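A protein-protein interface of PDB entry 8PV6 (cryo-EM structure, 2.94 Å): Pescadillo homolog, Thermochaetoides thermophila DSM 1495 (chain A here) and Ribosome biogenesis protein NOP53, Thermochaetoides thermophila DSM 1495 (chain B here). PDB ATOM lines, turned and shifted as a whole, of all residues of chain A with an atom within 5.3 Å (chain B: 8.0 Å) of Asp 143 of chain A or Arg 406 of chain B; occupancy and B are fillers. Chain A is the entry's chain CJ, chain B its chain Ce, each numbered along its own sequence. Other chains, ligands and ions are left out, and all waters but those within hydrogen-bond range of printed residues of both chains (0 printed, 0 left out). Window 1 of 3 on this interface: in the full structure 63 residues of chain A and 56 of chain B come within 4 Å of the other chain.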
ATOM      1  N   ASP A 140       9.791 -10.406  36.580  1.00  0.00           N
ATOM      2  CA  ASP A 140      10.305 -10.718  35.248  1.00  0.00           C
ATOM      3  C   ASP A 140       9.228 -10.623  34.171  1.00  0.00           C
ATOM      4  O   ASP A 140       9.531 -10.757  32.971  1.00  0.00           O
ATOM      5  CB  ASP A 140      10.942 -12.107  35.239  1.00  0.00           C
ATOM      6  CG  ASP A 140      12.133 -12.191  34.310  1.00  0.00           C
ATOM      7  OD1 ASP A 140      12.435 -11.183  33.639  1.00  0.00           O
ATOM      8  OD2 ASP A 140      12.772 -13.262  34.254  1.00  0.00           O
ATOM      9  N   LEU A 141       7.973 -10.398  34.576  1.00  0.00           N
ATOM     10  CA  LEU A 141       6.887 -10.225  33.620  1.00  0.00           C
ATOM     11  C   LEU A 141       7.079  -9.042  32.682  1.00  0.00           C
ATOM     12  O   LEU A 141       6.496  -9.057  31.599  1.00  0.00           O
ATOM     13  CB  LEU A 141       5.550 -10.063  34.339  1.00  0.00           C
ATOM     14  CG  LEU A 141       4.723 -11.329  34.541  1.00  0.00           C
ATOM     15  CD1 LEU A 141       3.350 -10.960  35.056  1.00  0.00           C
ATOM     16  CD2 LEU A 141       4.621 -12.113  33.248  1.00  0.00           C
ATOM     17  N   ASP A 142       7.871  -8.032  33.056  1.00  0.00           N
ATOM     18  CA  ASP A 142       8.132  -6.920  32.142  1.00  0.00           C
ATOM     19  C   ASP A 142       8.818  -7.407  30.871  1.00  0.00           C
ATOM     20  O   ASP A 142       8.328  -7.184  29.755  1.00  0.00           O
ATOM     21  CB  ASP A 142       8.995  -5.865  32.834  1.00  0.00           C
ATOM     22  CG  ASP A 142       8.360  -5.325  34.098  1.00  0.00           C
ATOM     23  OD1 ASP A 142       8.600  -5.902  35.179  1.00  0.00           O
ATOM     24  OD2 ASP A 142       7.633  -4.314  34.015  1.00  0.00           O
ATOM     25  N   ASP A 143       9.931  -8.127  31.034  1.00  0.00           N
ATOM     26  CA  ASP A 143      10.652  -8.681  29.895  1.00  0.00           C
ATOM     27  C   ASP A 143       9.829  -9.747  29.185  1.00  0.00           C
ATOM     28  O   ASP A 143       9.833  -9.821  27.948  1.00  0.00           O
ATOM     29  CB  ASP A 143      11.989  -9.254  30.360  1.00  0.00           C
ATOM     30  CG  ASP A 143      13.044  -9.217  29.280  1.00  0.00           C
ATOM     31  OD1 ASP A 143      12.715  -8.846  28.133  1.00  0.00           O
ATOM     32  OD2 ASP A 143      14.205  -9.562  29.580  1.00  0.00           O
ATOM     33  N   CYS A 144       9.111 -10.576  29.955  1.00  0.00           N
ATOM     34  CA  CYS A 144       8.287 -11.625  29.353  1.00  0.00           C
ATOM     35  C   CYS A 144       7.207 -11.045  28.444  1.00  0.00           C
ATOM     36  O   CYS A 144       7.050 -11.469  27.290  1.00  0.00           O
ATOM     37  CB  CYS A 144       7.654 -12.478  30.452  1.00  0.00           C
ATOM     38  SG  CYS A 144       6.428 -13.661  29.859  1.00  0.00           S
ATOM     39  N   LEU A 145       6.473 -10.047  28.943  1.00  0.00           N
ATOM     40  CA  LEU A 145       5.398  -9.440  28.174  1.00  0.00           C
ATOM     41  C   LEU A 145       5.936  -8.649  26.993  1.00  0.00           C
ATOM     42  O   LEU A 145       5.329  -8.662  25.918  1.00  0.00           O
ATOM     43  CB  LEU A 145       4.552  -8.546  29.075  1.00  0.00           C
ATOM     44  CG  LEU A 145       3.625  -9.267  30.050  1.00  0.00           C
ATOM     45  CD1 LEU A 145       3.165  -8.297  31.112  1.00  0.00           C
ATOM     46  CD2 LEU A 145       2.445  -9.872  29.316  1.00  0.00           C
ATOM     47  N   SER A 146       7.073  -7.962  27.166  1.00  0.00           N
ATOM     48  CA  SER A 146       7.666  -7.239  26.043  1.00  0.00           C
ATOM     49  C   SER A 146       8.050  -8.188  24.916  1.00  0.00           C
ATOM     50  O   SER A 146       7.699  -7.952  23.751  1.00  0.00           O
ATOM     51  CB  SER A 146       8.882  -6.447  26.513  1.00  0.00           C
ATOM     52  OG  SER A 146       8.499  -5.431  27.418  1.00  0.00           O
ATOM     53  N   MET A 147       8.719  -9.297  25.254  1.00  0.00           N
ATOM     54  CA  MET A 147       9.140 -10.259  24.240  1.00  0.00           C
ATOM     55  C   MET A 147       7.944 -10.910  23.552  1.00  0.00           C
ATOM     56  O   MET A 147       7.921 -11.041  22.321  1.00  0.00           O
ATOM     57  CB  MET A 147      10.041 -11.317  24.876  1.00  0.00           C
ATOM     58  CG  MET A 147      10.592 -12.338  23.902  1.00  0.00           C
ATOM     59  SD  MET A 147      11.694 -11.617  22.674  1.00  0.00           S
ATOM     60  CE  MET A 147      13.011 -11.016  23.723  1.00  0.00           C
ATOM     61  N   LEU A 148       6.921 -11.297  24.321  1.00  0.00           N
ATOM     62  CA  LEU A 148       5.801 -12.010  23.712  1.00  0.00           C
ATOM     63  C   LEU A 148       4.902 -11.078  22.904  1.00  0.00           C
ATOM     64  O   LEU A 148       4.397 -11.469  21.844  1.00  0.00           O
ATOM     65  CB  LEU A 148       5.001 -12.752  24.779  1.00  0.00           C
ATOM     66  CG  LEU A 148       5.744 -13.942  25.391  1.00  0.00           C
ATOM     67  CD1 LEU A 148       4.819 -14.736  26.280  1.00  0.00           C
ATOM     68  CD2 LEU A 148       6.342 -14.834  24.316  1.00  0.00           C
ATOM     69  N   LEU A 150       6.010  -8.472  21.374  1.00  0.00           N
ATOM     70  CA  LEU A 150       6.783  -8.255  20.157  1.00  0.00           C
ATOM     71  C   LEU A 150       6.612  -9.413  19.181  1.00  0.00           C
ATOM     72  O   LEU A 150       6.386  -9.204  17.984  1.00  0.00           O
ATOM     73  CB  LEU A 150       8.258  -8.063  20.506  1.00  0.00           C
ATOM     74  CG  LEU A 150       9.251  -8.037  19.346  1.00  0.00           C
ATOM     75  CD1 LEU A 150       8.936  -6.915  18.369  1.00  0.00           C
ATOM     76  CD2 LEU A 150      10.659  -7.910  19.883  1.00  0.00           C
ATOM     77  N   TYR A 234       9.587 -17.787  27.780  1.00  0.00           N
ATOM     78  CA  TYR A 234       8.670 -16.775  28.288  1.00  0.00           C
ATOM     79  C   TYR A 234       7.209 -17.162  28.092  1.00  0.00           C
ATOM     80  O   TYR A 234       6.369 -16.800  28.919  1.00  0.00           O
ATOM     81  CB  TYR A 234       8.973 -15.424  27.642  1.00  0.00           C
ATOM     82  CG  TYR A 234      10.182 -14.747  28.246  1.00  0.00           C
ATOM     83  CD1 TYR A 234      10.401 -14.777  29.617  1.00  0.00           C
ATOM     84  CD2 TYR A 234      11.105 -14.085  27.450  1.00  0.00           C
ATOM     85  CE1 TYR A 234      11.505 -14.164  30.178  1.00  0.00           C
ATOM     86  CE2 TYR A 234      12.212 -13.470  28.002  1.00  0.00           C
ATOM     87  CZ  TYR A 234      12.406 -13.513  29.367  1.00  0.00           C
ATOM     88  OH  TYR A 234      13.505 -12.901  29.922  1.00  0.00           O
ATOM     89  N   PRO B 204      17.451  -1.805  33.819  1.00  0.00           N
ATOM     90  CA  PRO B 204      16.128  -2.436  33.771  1.00  0.00           C
ATOM     91  C   PRO B 204      15.815  -2.968  32.383  1.00  0.00           C
ATOM     92  O   PRO B 204      16.356  -2.499  31.377  1.00  0.00           O
ATOM     93  CB  PRO B 204      15.175  -1.300  34.159  1.00  0.00           C
ATOM     94  CG  PRO B 204      16.039  -0.255  34.792  1.00  0.00           C
ATOM     95  CD  PRO B 204      17.364  -0.368  34.115  1.00  0.00           C
ATOM     96  N   ALA B 205      14.943  -3.979  32.344  1.00  0.00           N
ATOM     97  CA  ALA B 205      14.574  -4.601  31.076  1.00  0.00           C
ATOM     98  C   ALA B 205      13.834  -3.622  30.174  1.00  0.00           C
ATOM     99  O   ALA B 205      14.114  -3.531  28.973  1.00  0.00           O
ATOM    100  CB  ALA B 205      13.725  -5.846  31.332  1.00  0.00           C
ATOM    101  N   VAL B 206      12.883  -2.881  30.734  1.00  0.00           N
ATOM    102  CA  VAL B 206      12.180  -1.832  30.002  1.00  0.00           C
ATOM    103  C   VAL B 206      12.371  -0.519  30.750  1.00  0.00           C
ATOM    104  O   VAL B 206      11.737  -0.307  31.794  1.00  0.00           O
ATOM    105  CB  VAL B 206      10.688  -2.162  29.831  1.00  0.00           C
ATOM    106  CG1 VAL B 206       9.990  -1.057  29.060  1.00  0.00           C
ATOM    107  CG2 VAL B 206      10.515  -3.488  29.121  1.00  0.00           C
ATOM    108  N   PRO B 207      13.248   0.367  30.280  1.00  0.00           N
ATOM    109  CA  PRO B 207      13.419   1.662  30.950  1.00  0.00           C
ATOM    110  C   PRO B 207      12.174   2.527  30.816  1.00  0.00           C
ATOM    111  O   PRO B 207      11.430   2.430  29.838  1.00  0.00           O
ATOM    112  CB  PRO B 207      14.615   2.284  30.220  1.00  0.00           C
ATOM    113  CG  PRO B 207      15.317   1.130  29.579  1.00  0.00           C
ATOM    114  CD  PRO B 207      14.232   0.172  29.205  1.00  0.00           C
ATOM    115  N   ASP B 363      21.581   2.731  29.409  1.00  0.00           N
ATOM    116  CA  ASP B 363      21.931   2.059  28.163  1.00  0.00           C
ATOM    117  C   ASP B 363      22.736   2.965  27.235  1.00  0.00           C
ATOM    118  O   ASP B 363      23.461   2.462  26.372  1.00  0.00           O
ATOM    119  CB  ASP B 363      20.647   1.583  27.472  1.00  0.00           C
ATOM    120  CG  ASP B 363      20.868   0.409  26.522  1.00  0.00           C
ATOM    121  OD1 ASP B 363      22.015   0.136  26.116  1.00  0.00           O
ATOM    122  OD2 ASP B 363      19.868  -0.254  26.175  1.00  0.00           O
ATOM    123  N   ASN B 401      14.088  -0.331  16.046  1.00  0.00           N
ATOM    124  CA  ASN B 401      13.661  -1.714  15.880  1.00  0.00           C
ATOM    125  C   ASN B 401      13.560  -2.337  17.261  1.00  0.00           C
ATOM    126  O   ASN B 401      14.551  -2.375  17.998  1.00  0.00           O
ATOM    127  CB  ASN B 401      14.641  -2.494  14.996  1.00  0.00           C
ATOM    128  CG  ASN B 401      14.072  -3.813  14.506  1.00  0.00           C
ATOM    129  OD1 ASN B 401      13.668  -4.666  15.294  1.00  0.00           O
ATOM    130  ND2 ASN B 401      14.040  -3.985  13.190  1.00  0.00           N
ATOM    131  N   LEU B 402      12.367  -2.827  17.608  1.00  0.00           N
ATOM    132  CA  LEU B 402      12.148  -3.345  18.955  1.00  0.00           C
ATOM    133  C   LEU B 402      12.868  -4.669  19.168  1.00  0.00           C
ATOM    134  O   LEU B 402      13.310  -4.962  20.284  1.00  0.00           O
ATOM    135  CB  LEU B 402      10.652  -3.490  19.230  1.00  0.00           C
ATOM    136  CG  LEU B 402       9.833  -2.197  19.273  1.00  0.00           C
ATOM    137  CD1 LEU B 402       8.534  -2.429  20.010  1.00  0.00           C
ATOM    138  CD2 LEU B 402      10.607  -1.055  19.918  1.00  0.00           C
ATOM    139  N   LEU B 403      12.998  -5.480  18.117  1.00  0.00           N
ATOM    140  CA  LEU B 403      13.747  -6.729  18.234  1.00  0.00           C
ATOM    141  C   LEU B 403      15.223  -6.462  18.504  1.00  0.00           C
ATOM    142  O   LEU B 403      15.841  -7.121  19.354  1.00  0.00           O
ATOM    143  CB  LEU B 403      13.564  -7.561  16.967  1.00  0.00           C
ATOM    144  CG  LEU B 403      14.082  -8.997  16.995  1.00  0.00           C
ATOM    145  CD1 LEU B 403      13.460  -9.759  18.150  1.00  0.00           C
ATOM    146  CD2 LEU B 403      13.779  -9.686  15.677  1.00  0.00           C
ATOM    147  N   LYS B 404      15.798  -5.476  17.813  1.00  0.00           N
ATOM    148  CA  LYS B 404      17.181  -5.095  18.077  1.00  0.00           C
ATOM    149  C   LYS B 404      17.319  -4.456  19.453  1.00  0.00           C
ATOM    150  O   LYS B 404      18.353  -4.611  20.114  1.00  0.00           O
ATOM    151  CB  LYS B 404      17.680  -4.148  16.986  1.00  0.00           C
ATOM    152  CG  LYS B 404      19.180  -3.938  16.986  1.00  0.00           C
ATOM    153  CD  LYS B 404      19.614  -3.091  15.805  1.00  0.00           C
ATOM    154  CE  LYS B 404      21.125  -2.953  15.754  1.00  0.00           C
ATOM    155  NZ  LYS B 404      21.562  -2.089  14.624  1.00  0.00           N
ATOM    156  N   ASP B 405      16.284  -3.742  19.906  1.00  0.00           N
ATOM    157  CA  ASP B 405      16.301  -3.185  21.255  1.00  0.00           C
ATOM    158  C   ASP B 405      16.307  -4.284  22.311  1.00  0.00           C
ATOM    159  O   ASP B 405      17.028  -4.187  23.310  1.00  0.00           O
ATOM    160  CB  ASP B 405      15.107  -2.254  21.459  1.00  0.00           C
ATOM    161  CG  ASP B 405      15.265  -0.936  20.730  1.00  0.00           C
ATOM    162  OD1 ASP B 405      16.394  -0.628  20.298  1.00  0.00           O
ATOM    163  OD2 ASP B 405      14.260  -0.206  20.594  1.00  0.00           O
ATOM    164  N   ARG B 406      15.516  -5.341  22.105  1.00  0.00           N
ATOM    165  CA  ARG B 406      15.519  -6.464  23.041  1.00  0.00           C
ATOM    166  C   ARG B 406      16.852  -7.202  23.016  1.00  0.00           C
ATOM    167  O   ARG B 406      17.348  -7.635  24.063  1.00  0.00           O
ATOM    168  CB  ARG B 406      14.371  -7.425  22.728  1.00  0.00           C
ATOM    169  CG  ARG B 406      12.978  -6.832  22.884  1.00  0.00           C
ATOM    170  CD  ARG B 406      12.315  -7.208  24.203  1.00  0.00           C
ATOM    171  NE  ARG B 406      13.139  -6.904  25.367  1.00  0.00           N
ATOM    172  CZ  ARG B 406      13.243  -5.703  25.920  1.00  0.00           C
ATOM    173  NH1 ARG B 406      12.599  -4.657  25.430  1.00  0.00           N
ATOM    174  NH2 ARG B 406      14.016  -5.547  26.991  1.00  0.00           N
ATOM    175  N   TYR B 407      17.447  -7.350  21.827  1.00  0.00           N
ATOM    176  CA  TYR B 407      18.763  -7.980  21.720  1.00  0.00           C
ATOM    177  C   TYR B 407      19.828  -7.174  22.461  1.00  0.00           C
ATOM    178  O   TYR B 407      20.639  -7.738  23.212  1.00  0.00           O
ATOM    179  CB  TYR B 407      19.129  -8.139  20.245  1.00  0.00           C
ATOM    180  CG  TYR B 407      20.339  -9.000  19.973  1.00  0.00           C
ATOM    181  CD1 TYR B 407      20.360 -10.337  20.338  1.00  0.00           C
ATOM    182  CD2 TYR B 407      21.449  -8.479  19.324  1.00  0.00           C
ATOM    183  CE1 TYR B 407      21.461 -11.129  20.082  1.00  0.00           C
ATOM    184  CE2 TYR B 407      22.554  -9.263  19.062  1.00  0.00           C
ATOM    185  CZ  TYR B 407      22.554 -10.587  19.446  1.00  0.00           C
ATOM    186  OH  TYR B 407      23.654 -11.372  19.188  1.00  0.00           O
ATOM    187  N   ARG B 408      19.821  -5.849  22.280  1.00  0.00           N
ATOM    188  CA  ARG B 408      20.752  -4.986  22.998  1.00  0.00           C
ATOM    189  C   ARG B 408      20.503  -5.026  24.498  1.00  0.00           C
ATOM    190  O   ARG B 408      21.450  -4.970  25.287  1.00  0.00           O
ATOM    191  CB  ARG B 408      20.648  -3.551  22.487  1.00  0.00           C
ATOM    192  CG  ARG B 408      21.388  -3.287  21.191  1.00  0.00           C
ATOM    193  CD  ARG B 408      21.431  -1.798  20.906  1.00  0.00           C
ATOM    194  NE  ARG B 408      21.918  -1.048  22.056  1.00  0.00           N
ATOM    195  CZ  ARG B 408      23.177  -0.668  22.225  1.00  0.00           C
ATOM    196  NH1 ARG B 408      24.108  -0.946  21.327  1.00  0.00           N
ATOM    197  NH2 ARG B 408      23.510   0.008  23.320  1.00  0.00           N
ATOM    198  N   SER B 409      19.235  -5.114  24.908  1.00  0.00           N
ATOM    199  CA  SER B 409      18.915  -5.222  26.328  1.00  0.00           C
ATOM    200  C   SER B 409      19.467  -6.508  26.925  1.00  0.00           C
ATOM    201  O   SER B 409      20.012  -6.499  28.034  1.00  0.00           O
ATOM    202  CB  SER B 409      17.405  -5.145  26.532  1.00  0.00           C
ATOM    203  OG  SER B 409      17.069  -5.329  27.895  1.00  0.00           O
ATOM    204  N   MET B 410      19.340  -7.623  26.198  1.00  0.00           N
ATOM    205  CA  MET B 410      19.892  -8.890  26.673  1.00  0.00           C
ATOM    206  C   MET B 410      21.410  -8.827  26.796  1.00  0.00           C
ATOM    207  O   MET B 410      21.976  -9.296  27.792  1.00  0.00           O
ATOM    208  CB  MET B 410      19.488 -10.033  25.743  1.00  0.00           C
ATOM    209  CG  MET B 410      18.003 -10.335  25.700  1.00  0.00           C
ATOM    210  SD  MET B 410      17.346 -10.907  27.275  1.00  0.00           S
ATOM    211  CE  MET B 410      15.594 -10.925  26.908  1.00  0.00           C
ATOM    212  N   ILE B 411      22.086  -8.237  25.804  1.00  0.00           N
ATOM    213  CA  ILE B 411      23.546  -8.165  25.858  1.00  0.00           C
ATOM    214  C   ILE B 411      24.004  -7.238  26.981  1.00  0.00           C
ATOM    215  O   ILE B 411      24.950  -7.549  27.714  1.00  0.00           O
ATOM    216  CB  ILE B 411      24.126  -7.735  24.498  1.00  0.00           C
ATOM    217  CG1 ILE B 411      23.714  -8.720  23.408  1.00  0.00           C
ATOM    218  CG2 ILE B 411      25.644  -7.668  24.562  1.00  0.00           C
ATOM    219  CD1 ILE B 411      24.290  -8.392  22.053  1.00  0.00           C
ATOM    220  N   VAL B 412      23.332  -6.092  27.143  1.00  0.00           N
ATOM    221  CA  VAL B 412      23.698  -5.135  28.185  1.00  0.00           C
ATOM    222  C   VAL B 412      23.457  -5.711  29.574  1.00  0.00           C
ATOM    223  O   VAL B 412      24.314  -5.596  30.459  1.00  0.00           O
ATOM    224  CB  VAL B 412      22.939  -3.809  27.966  1.00  0.00           C
ATOM    225  CG1 VAL B 412      22.924  -2.970  29.229  1.00  0.00           C
ATOM    226  CG2 VAL B 412      23.581  -3.024  26.839  1.00  0.00           C
ATOM    227  N   ARG B 413      22.318  -6.367  29.788  1.00  0.00           N
ATOM    228  CA  ARG B 413      22.028  -6.995  31.068  1.00  0.00           C
ATOM    229  C   ARG B 413      22.817  -8.278  31.290  1.00  0.00           C
ATOM    230  O   ARG B 413      22.816  -8.799  32.409  1.00  0.00           O
ATOM    231  CB  ARG B 413      20.531  -7.279  31.185  1.00  0.00           C
ATOM    232  CG  ARG B 413      19.686  -6.027  31.328  1.00  0.00           C
ATOM    233  CD  ARG B 413      18.225  -6.376  31.496  1.00  0.00           C
ATOM    234  NE  ARG B 413      17.664  -6.944  30.279  1.00  0.00           N
ATOM    235  CZ  ARG B 413      16.697  -7.849  30.256  1.00  0.00           C
ATOM    236  NH1 ARG B 413      16.166  -8.320  31.372  1.00  0.00           N
ATOM    237  NH2 ARG B 413      16.252  -8.295  29.085  1.00  0.00           N
ATOM    238  N   LYS B 415      22.641 -11.453  29.960  1.00  0.00           N
ATOM    239  CA  LYS B 415      22.089 -12.798  29.864  1.00  0.00           C
ATOM    240  C   LYS B 415      22.731 -13.596  28.738  1.00  0.00           C
ATOM    241  O   LYS B 415      22.646 -14.828  28.731  1.00  0.00           O
ATOM    242  CB  LYS B 415      20.573 -12.733  29.679  1.00  0.00           C
ATOM    243  CG  LYS B 415      19.850 -12.086  30.846  1.00  0.00           C
ATOM    244  CD  LYS B 415      18.349 -12.120  30.663  1.00  0.00           C
ATOM    245  CE  LYS B 415      17.642 -11.553  31.880  1.00  0.00           C
ATOM    246  NZ  LYS B 415      16.163 -11.556  31.715  1.00  0.00           N
ATOM    247  N   LEU B 416      23.377 -12.919  27.791  1.00  0.00           N
ATOM    248  CA  LEU B 416      24.106 -13.586  26.724  1.00  0.00           C
ATOM    249  C   LEU B 416      25.224 -12.664  26.259  1.00  0.00           C
ATOM    250  O   LEU B 416      25.323 -11.511  26.681  1.00  0.00           O
ATOM    251  CB  LEU B 416      23.168 -13.998  25.576  1.00  0.00           C
ATOM    252  CG  LEU B 416      22.320 -12.982  24.801  1.00  0.00           C
ATOM    253  CD1 LEU B 416      23.058 -12.361  23.624  1.00  0.00           C
ATOM    254  CD2 LEU B 416      21.040 -13.637  24.327  1.00  0.00           C
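The guanidinium group (NH2) of Arg 406 of chain B is in hydrogen-bond range of the side-chain hydroxyl (OG) of Ser 409 of chain B (3.2 Å). The side-chain amide oxygen (OD1) of Asn 401 of chain B lies within hydrogen-bond range of the backbone NH (N) of Leu 403 of chain B (3.0 Å). N of Lys 415 of chain B lies within hydrogen-bond range of O of Met 410 of chain B (3.1 Å). The side-chain hydroxyl of Ser 146 of chain A is in hydrogen-bond range of the backbone carbonyl oxygen of Asp 142 of chain A (2.9 Å). NH2 of Arg 406 of chain B sits at hydrogen-bond distance from O of Ala 205 of chain B, 2.8 Å away. O of Tyr 234 of chain A lies within hydrogen-bond range of SG of Cys 144 of chain A, 3.3 Å away.
Printed residues of chain A that touch a printed residue of chain B: Asp 143, Ser 146, Met 147, Leu 150 and Tyr 234. Of the 20 printed residues of chain B, 8 touch a printed residue of chain A. Printed residues of chain B that touch a printed residue of chain A: Ala 205, Val 206, Leu 402, Leu 403, Arg 406, Met 410, Arg 413 and Lys 415. Hydrophobic or aromatic side chains of chain B that line the printed part of chain A: Ala 205, Val 206, Leu 402, Leu 403 and Met 410. Among the printed residues, Asp or Glu carboxylates within 4 Å of a Lys or Arg side-chain nitrogen of the other chain: Asp 143 of chain A with Arg 406 of chain B (3.4 Å), Asp 143 of chain A with Arg 413 of chain B (2.5 Å) and Asp 143 of chain A with Lys 415 of chain B (3.5 Å).
Arg 406 of chain B touches three residues of chain A. Of the printed residues of chain A, Leu 403 of chain B touches Leu 150. Printed residues of chain A within 4 Å of Met 410 of chain B: Asp 143 (3.3 Å). Printed residues of chain A within 4 Å of Val 206 of chain B: Ser 146 (3.3 Å). Printed residues of chain B within 4 Å of Met 147 of chain A: Arg 406 (3.9 Å). Val 412 of chain B touches none of the printed residues of chain A. Asp 140 of chain A touches none of the printed residues of chain B.
The side-chain amino group of Lys 415 of chain B lies within hydrogen-bond range of the side-chain hydroxyl of Tyr 234 of chain A, 3.5 Å away. The side-chain carboxylate of Asp 143 of chain A is in salt-bridge range of the guanidinium group of Arg 413 of chain B, at 2.5 Å. The guanidinium group of Arg 406 of chain B lies within salt-bridge range of the side-chain carboxylate of Asp 143 of chain A (3.4 Å). The side-chain amino group (NZ) of Lys 415 of chain B lies within salt-bridge range of the side-chain carboxylate (OD2) of Asp 143 of chain A (3.5 Å).
Asp 143 of chain A touches Ala 205 of chain B. OD2 of Asp 143 of chain A touches CE of Met 410 of chain B, 3.3 Å away. CG2 of Val 206 of chain B touches OG of Ser 146 of chain A (3.3 Å). CD of Arg 406 of chain B touches CE of Met 147 of chain A (3.9 Å). CD1 of Leu 150 of chain A touches CB of Leu 402 of chain B, 3.9 Å away. Leu 150 of chain A touches Leu 403 of chain B (CD2 to CA, 3.7 Å). Leu 150 of chain A touches Arg 406 of chain B (CD2 to CG, 3.9 Å).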
